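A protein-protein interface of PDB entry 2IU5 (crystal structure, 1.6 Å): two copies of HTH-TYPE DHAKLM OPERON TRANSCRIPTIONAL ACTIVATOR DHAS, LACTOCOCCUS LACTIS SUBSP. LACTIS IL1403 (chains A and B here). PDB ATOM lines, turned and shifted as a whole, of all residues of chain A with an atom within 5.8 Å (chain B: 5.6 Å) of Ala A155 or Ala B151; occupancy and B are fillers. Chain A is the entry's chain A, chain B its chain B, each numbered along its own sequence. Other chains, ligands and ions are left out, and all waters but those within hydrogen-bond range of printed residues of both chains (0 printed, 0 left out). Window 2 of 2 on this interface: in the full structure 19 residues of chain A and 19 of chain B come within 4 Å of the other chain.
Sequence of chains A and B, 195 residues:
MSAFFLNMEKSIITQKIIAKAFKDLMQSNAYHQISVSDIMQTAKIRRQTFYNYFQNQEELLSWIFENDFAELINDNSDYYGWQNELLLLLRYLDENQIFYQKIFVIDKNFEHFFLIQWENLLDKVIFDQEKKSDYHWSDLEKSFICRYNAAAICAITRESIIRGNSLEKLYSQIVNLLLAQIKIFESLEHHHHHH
Of the printed residues of chain B, Ala A151 touches Ala B155.
Of the printed residues of chain B, Ala A152 touches Tyr B148 (3.3 Å) and Ala B152 (3.9 Å).
Printed residues of chain B within 4 Å of Ile A153: Tyr B148.
Ala A155 touches just one residue of chain B: Ala B151 (3.7 Å).
Thr A157 touches none of the printed residues of chain B.
Ser A160 touches none of the printed residues of chain B.
Printed residues of chain A within 4 Å of Tyr B148: Ala A152 and Ile A153.
Of the printed residues of chain A, Ala B155 touches Ala A151.
Ala A151 touches Ala B155 (CB to CB, 3.4 Å).
CB of Ala A152 touches O of Tyr B148 (3.3 Å).
Ala A152 touches Ala B152 (CB to CB, 3.9 Å).
Ile A153 touches Tyr B148.
CB of Ala A155 touches CB of Ala B151, at 3.7 Å.
Of the 11 printed residues of chain A, 4 touch a printed residue of chain B.
Hydrophobic or aromatic side chains of chain A within 4 Å of the printed part of chain B: Ala A151, Ala A152, Ile A153 and Ala A155.
Of the 12 printed residues of chain B, 4 touch a printed residue of chain A.
Hydrophobic or aromatic side chains of chain B within 4 Å of the printed part of chain A: Tyr B148, Ala B151, Ala B152 and Ala B155.
Among the printed residues, 5 pairs touch across the chains.
O of Ile A153 sits at hydrogen-bond distance from OG1 of Thr A157 (2.8 Å).
Ala A151 touches Ala B155, and with the chains exchanged Ala A155 touches Ala B151.
Ala B152 touches its own counterpart, Ala A152.
Positions printed for both chains: 150, 151, 152, 153, 154, 155 and 156.
Of the 5 pairs that touch across the chains among the printed residues, 3 have their exchanged pair printed and touching as well.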
ATOM      1  N   ALA A 150      13.802   3.789  -3.933  1.00  0.00           N
ATOM      2  CA  ALA A 150      12.539   4.441  -3.592  1.00  0.00           C
ATOM      3  C   ALA A 150      11.475   3.360  -3.377  1.00  0.00           C
ATOM      4  O   ALA A 150      10.661   3.431  -2.431  1.00  0.00           O
ATOM      5  CB  ALA A 150      12.161   5.395  -4.709  1.00  0.00           C
ATOM      6  N   ALA A 151      11.473   2.350  -4.241  1.00  0.00           N
ATOM      7  CA  ALA A 151      10.455   1.296  -4.158  1.00  0.00           C
ATOM      8  C   ALA A 151      10.611   0.504  -2.872  1.00  0.00           C
ATOM      9  O   ALA A 151       9.615   0.177  -2.211  1.00  0.00           O
ATOM     10  CB  ALA A 151      10.522   0.361  -5.374  1.00  0.00           C
ATOM     11  N   ALA A 152      11.855   0.200  -2.529  1.00  0.00           N
ATOM     12  CA  ALA A 152      12.138  -0.533  -1.286  1.00  0.00           C
ATOM     13  C   ALA A 152      11.692   0.268  -0.075  1.00  0.00           C
ATOM     14  O   ALA A 152      10.964  -0.240   0.775  1.00  0.00           O
ATOM     15  CB  ALA A 152      13.609  -0.853  -1.173  1.00  0.00           C
ATOM     16  N   ILE A 153      12.118   1.517   0.013  1.00  0.00           N
ATOM     17  CA  ILE A 153      11.772   2.299   1.184  1.00  0.00           C
ATOM     18  C   ILE A 153      10.267   2.574   1.234  1.00  0.00           C
ATOM     19  O   ILE A 153       9.673   2.572   2.312  1.00  0.00           O
ATOM     20  CB  ILE A 153      12.600   3.579   1.268  1.00  0.00           C
ATOM     21  CG1 ILE A 153      14.100   3.248   1.266  1.00  0.00           C
ATOM     22  CG2 ILE A 153      12.165   4.357   2.504  1.00  0.00           C
ATOM     23  CD1 ILE A 153      15.007   4.438   0.906  1.00  0.00           C
ATOM     24  N   CYS A 154       9.640   2.801   0.082  1.00  0.00           N
ATOM     25  CA  CYS A 154       8.203   3.030   0.054  1.00  0.00           C
ATOM     26  C   CYS A 154       7.473   1.828   0.650  1.00  0.00           C
ATOM     27  O   CYS A 154       6.567   1.968   1.483  1.00  0.00           O
ATOM     28  CB  CYS A 154       7.761   3.275  -1.391  1.00  0.00           C
ATOM     29  SG  CYS A 154       5.998   3.574  -1.577  1.00  0.00           S
ATOM     30  N   ALA A 155       7.866   0.629   0.224  1.00  0.00           N
ATOM     31  CA  ALA A 155       7.190  -0.591   0.655  1.00  0.00           C
ATOM     32  C   ALA A 155       7.379  -0.840   2.151  1.00  0.00           C
ATOM     33  O   ALA A 155       6.440  -1.202   2.861  1.00  0.00           O
ATOM     34  CB  ALA A 155       7.717  -1.786  -0.137  1.00  0.00           C
ATOM     35  N   ILE A 156       8.606  -0.645   2.618  1.00  0.00           N
ATOM     36  CA  ILE A 156       8.955  -0.919   4.004  1.00  0.00           C
ATOM     37  C   ILE A 156       8.239   0.080   4.911  1.00  0.00           C
ATOM     38  O   ILE A 156       7.679  -0.305   5.941  1.00  0.00           O
ATOM     39  CB  ILE A 156      10.466  -0.804   4.215  1.00  0.00           C
ATOM     40  CG1 ILE A 156      11.185  -1.977   3.535  1.00  0.00           C
ATOM     41  CG2 ILE A 156      10.779  -0.711   5.698  1.00  0.00           C
ATOM     42  CD1 ILE A 156      10.938  -3.287   4.193  1.00  0.00           C
ATOM     43  N   THR A 157       8.246   1.350   4.535  1.00  0.00           N
ATOM     44  CA  THR A 157       7.655   2.369   5.410  1.00  0.00           C
ATOM     45  C   THR A 157       6.135   2.315   5.385  1.00  0.00           C
ATOM     46  O   THR A 157       5.494   2.457   6.425  1.00  0.00           O
ATOM     47  CB  THR A 157       8.167   3.789   5.100  1.00  0.00           C
ATOM     48  OG1 THR A 157       7.837   4.129   3.747  1.00  0.00           O
ATOM     49  CG2 THR A 157       9.659   3.872   5.325  1.00  0.00           C
ATOM     50  N   ARG A 158       5.534   2.095   4.214  1.00  0.00           N
ATOM     51  CA  ARG A 158       4.095   1.838   4.178  1.00  0.00           C
ATOM     52  C   ARG A 158       3.691   0.689   5.096  1.00  0.00           C
ATOM     53  O   ARG A 158       2.746   0.811   5.876  1.00  0.00           O
ATOM     54  CB  ARG A 158       3.607   1.543   2.754  1.00  0.00           C
ATOM     55  CG  ARG A 158       2.118   1.162   2.718  1.00  0.00           C
ATOM     56  CD  ARG A 158       1.615   0.907   1.290  1.00  0.00           C
ATOM     57  NE  ARG A 158       0.252   0.377   1.237  1.00  0.00           N
ATOM     58  CZ  ARG A 158      -0.078  -0.898   1.424  1.00  0.00           C
ATOM     59  NH1 ARG A 158       0.851  -1.814   1.684  1.00  0.00           N
ATOM     60  NH2 ARG A 158      -1.356  -1.263   1.350  1.00  0.00           N
ATOM     61  N   GLU A 159       4.390  -0.433   5.014  1.00  0.00           N
ATOM     62  CA  GLU A 159       4.038  -1.577   5.858  1.00  0.00           C
ATOM     63  C   GLU A 159       4.187  -1.234   7.336  1.00  0.00           C
ATOM     64  O   GLU A 159       3.333  -1.589   8.143  1.00  0.00           O
ATOM     65  CB  GLU A 159       4.881  -2.800   5.507  1.00  0.00           C
ATOM     66  CG  GLU A 159       4.613  -3.984   6.416  1.00  0.00           C
ATOM     67  CD  GLU A 159       5.508  -5.168   6.092  1.00  0.00           C
ATOM     68  OE1 GLU A 159       6.648  -4.931   5.625  1.00  0.00           O
ATOM     69  OE2 GLU A 159       5.069  -6.320   6.303  1.00  0.00           O
ATOM     70  N   SER A 160       5.261  -0.545   7.696  1.00  0.00           N
ATOM     71  CA  SER A 160       5.497  -0.195   9.097  1.00  0.00           C
ATOM     72  C   SER A 160       4.390   0.738   9.602  1.00  0.00           C
ATOM     73  O   SER A 160       3.893   0.593  10.722  1.00  0.00           O
ATOM     74  CB  SER A 160       6.823   0.532   9.189  1.00  0.00           C
ATOM     75  OG  SER A 160       7.854  -0.401   8.927  1.00  0.00           O
ATOM     76  N   LEU B 115       5.815 -11.032  -5.085  1.00  0.00           N
ATOM     77  CA  LEU B 115       6.691 -10.567  -4.008  1.00  0.00           C
ATOM     78  C   LEU B 115       7.250 -11.742  -3.213  1.00  0.00           C
ATOM     79  O   LEU B 115       8.433 -11.768  -2.884  1.00  0.00           O
ATOM     80  CB  LEU B 115       5.922  -9.660  -3.050  1.00  0.00           C
ATOM     81  CG  LEU B 115       6.779  -9.150  -1.891  1.00  0.00           C
ATOM     82  CD1 LEU B 115       7.961  -8.275  -2.377  1.00  0.00           C
ATOM     83  CD2 LEU B 115       5.838  -8.344  -1.026  1.00  0.00           C
ATOM     84  N   CYS B 146      16.743  -8.818   3.158  1.00  0.00           N
ATOM     85  CA  CYS B 146      15.843  -9.619   2.328  1.00  0.00           C
ATOM     86  C   CYS B 146      14.516  -8.914   2.038  1.00  0.00           C
ATOM     87  O   CYS B 146      14.072  -8.874   0.882  1.00  0.00           O
ATOM     88  CB  CYS B 146      15.558 -10.942   3.028  1.00  0.00           C
ATOM     89  SG  CYS B 146      16.959 -12.067   3.051  1.00  0.00           S
ATOM     90  N   ARG B 147      13.879  -8.359   3.070  1.00  0.00           N
ATOM     91  CA  ARG B 147      12.635  -7.624   2.856  1.00  0.00           C
ATOM     92  C   ARG B 147      12.834  -6.408   1.948  1.00  0.00           C
ATOM     93  O   ARG B 147      12.052  -6.163   1.030  1.00  0.00           O
ATOM     94  CB  ARG B 147      12.003  -7.199   4.187  1.00  0.00           C
ATOM     95  CG  ARG B 147      11.361  -8.359   4.932  1.00  0.00           C
ATOM     96  CD  ARG B 147      11.535  -8.213   6.446  1.00  0.00           C
ATOM     97  NE  ARG B 147      11.279  -6.857   6.934  1.00  0.00           N
ATOM     98  CZ  ARG B 147      11.827  -6.345   8.033  1.00  0.00           C
ATOM     99  NH1 ARG B 147      12.665  -7.075   8.763  1.00  0.00           N
ATOM    100  NH2 ARG B 147      11.535  -5.101   8.402  1.00  0.00           N
ATOM    101  N   TYR B 148      13.895  -5.650   2.217  1.00  0.00           N
ATOM    102  CA  TYR B 148      14.171  -4.431   1.452  1.00  0.00           C
ATOM    103  C   TYR B 148      14.393  -4.741  -0.015  1.00  0.00           C
ATOM    104  O   TYR B 148      13.793  -4.130  -0.882  1.00  0.00           O
ATOM    105  CB  TYR B 148      15.417  -3.787   2.039  1.00  0.00           C
ATOM    106  CG  TYR B 148      15.827  -2.417   1.521  1.00  0.00           C
ATOM    107  CD1 TYR B 148      15.440  -1.277   2.218  1.00  0.00           C
ATOM    108  CD2 TYR B 148      16.599  -2.271   0.366  1.00  0.00           C
ATOM    109  CE1 TYR B 148      15.800  -0.022   1.778  1.00  0.00           C
ATOM    110  CE2 TYR B 148      16.973  -1.010  -0.098  1.00  0.00           C
ATOM    111  CZ  TYR B 148      16.568   0.105   0.619  1.00  0.00           C
ATOM    112  OH  TYR B 148      16.931   1.367   0.184  1.00  0.00           O
ATOM    113  N   ASN B 149      15.270  -5.702  -0.286  1.00  0.00           N
ATOM    114  CA  ASN B 149      15.618  -6.002  -1.663  1.00  0.00           C
ATOM    115  C   ASN B 149      14.546  -6.766  -2.410  1.00  0.00           C
ATOM    116  O   ASN B 149      14.383  -6.581  -3.621  1.00  0.00           O
ATOM    117  CB  ASN B 149      16.983  -6.666  -1.702  1.00  0.00           C
ATOM    118  CG  ASN B 149      18.073  -5.649  -1.422  1.00  0.00           C
ATOM    119  OD1 ASN B 149      18.442  -4.877  -2.312  1.00  0.00           O
ATOM    120  ND2 ASN B 149      18.586  -5.636  -0.186  1.00  0.00           N
ATOM    121  N   ALA B 150      13.807  -7.615  -1.699  1.00  0.00           N
ATOM    122  CA  ALA B 150      12.705  -8.308  -2.352  1.00  0.00           C
ATOM    123  C   ALA B 150      11.674  -7.297  -2.833  1.00  0.00           C
ATOM    124  O   ALA B 150      11.200  -7.396  -3.958  1.00  0.00           O
ATOM    125  CB  ALA B 150      12.067  -9.342  -1.428  1.00  0.00           C
ATOM    126  N   ALA B 151      11.329  -6.326  -1.987  1.00  0.00           N
ATOM    127  CA  ALA B 151      10.412  -5.259  -2.379  1.00  0.00           C
ATOM    128  C   ALA B 151      10.945  -4.475  -3.578  1.00  0.00           C
ATOM    129  O   ALA B 151      10.198  -4.131  -4.471  1.00  0.00           O
ATOM    130  CB  ALA B 151      10.209  -4.305  -1.195  1.00  0.00           C
ATOM    131  N   ALA B 152      12.239  -4.189  -3.587  1.00  0.00           N
ATOM    132  CA  ALA B 152      12.830  -3.392  -4.660  1.00  0.00           C
ATOM    133  C   ALA B 152      12.751  -4.160  -5.967  1.00  0.00           C
ATOM    134  O   ALA B 152      12.272  -3.638  -6.975  1.00  0.00           O
ATOM    135  CB  ALA B 152      14.270  -3.079  -4.325  1.00  0.00           C
ATOM    136  N   ILE B 153      13.232  -5.403  -5.933  1.00  0.00           N
ATOM    137  CA  ILE B 153      13.256  -6.205  -7.150  1.00  0.00           C
ATOM    138  C   ILE B 153      11.842  -6.474  -7.665  1.00  0.00           C
ATOM    139  O   ILE B 153      11.582  -6.429  -8.869  1.00  0.00           O
ATOM    140  CB  ILE B 153      14.065  -7.516  -6.963  1.00  0.00           C
ATOM    141  CG1 ILE B 153      15.520  -7.174  -6.621  1.00  0.00           C
ATOM    142  CG2 ILE B 153      13.988  -8.325  -8.241  1.00  0.00           C
ATOM    143  CD1 ILE B 153      16.366  -8.341  -6.127  1.00  0.00           C
ATOM    144  N   CYS B 154      10.918  -6.755  -6.752  1.00  0.00           N
ATOM    145  CA  CYS B 154       9.520  -6.941  -7.128  1.00  0.00           C
ATOM    146  C   CYS B 154       8.988  -5.743  -7.908  1.00  0.00           C
ATOM    147  O   CYS B 154       8.396  -5.897  -8.974  1.00  0.00           O
ATOM    148  CB  CYS B 154       8.688  -7.183  -5.868  1.00  0.00           C
ATOM    149  SG  CYS B 154       6.975  -7.608  -6.235  1.00  0.00           S
ATOM    150  N   ALA B 155       9.198  -4.544  -7.383  1.00  0.00           N
ATOM    151  CA  ALA B 155       8.681  -3.337  -8.007  1.00  0.00           C
ATOM    152  C   ALA B 155       9.354  -3.067  -9.346  1.00  0.00           C
ATOM    153  O   ALA B 155       8.703  -2.683 -10.310  1.00  0.00           O
ATOM    154  CB  ALA B 155       8.879  -2.149  -7.058  1.00  0.00           C
ATOM    155  N   ILE B 156      10.663  -3.271  -9.400  1.00  0.00           N
ATOM    156  CA  ILE B 156      11.438  -2.894 -10.564  1.00  0.00           C
ATOM    157  C   ILE B 156      11.162  -3.845 -11.721  1.00  0.00           C
ATOM    158  O   ILE B 156      11.099  -3.428 -12.876  1.00  0.00           O
ATOM    159  CB  ILE B 156      12.926  -2.883 -10.204  1.00  0.00           C
ATOM    160  CG1 ILE B 156      13.250  -1.628  -9.400  1.00  0.00           C
ATOM    161  CG2 ILE B 156      13.806  -3.176 -11.418  1.00  0.00           C
ATOM    162  CD1 ILE B 156      13.294  -0.381 -10.252  1.00  0.00           C
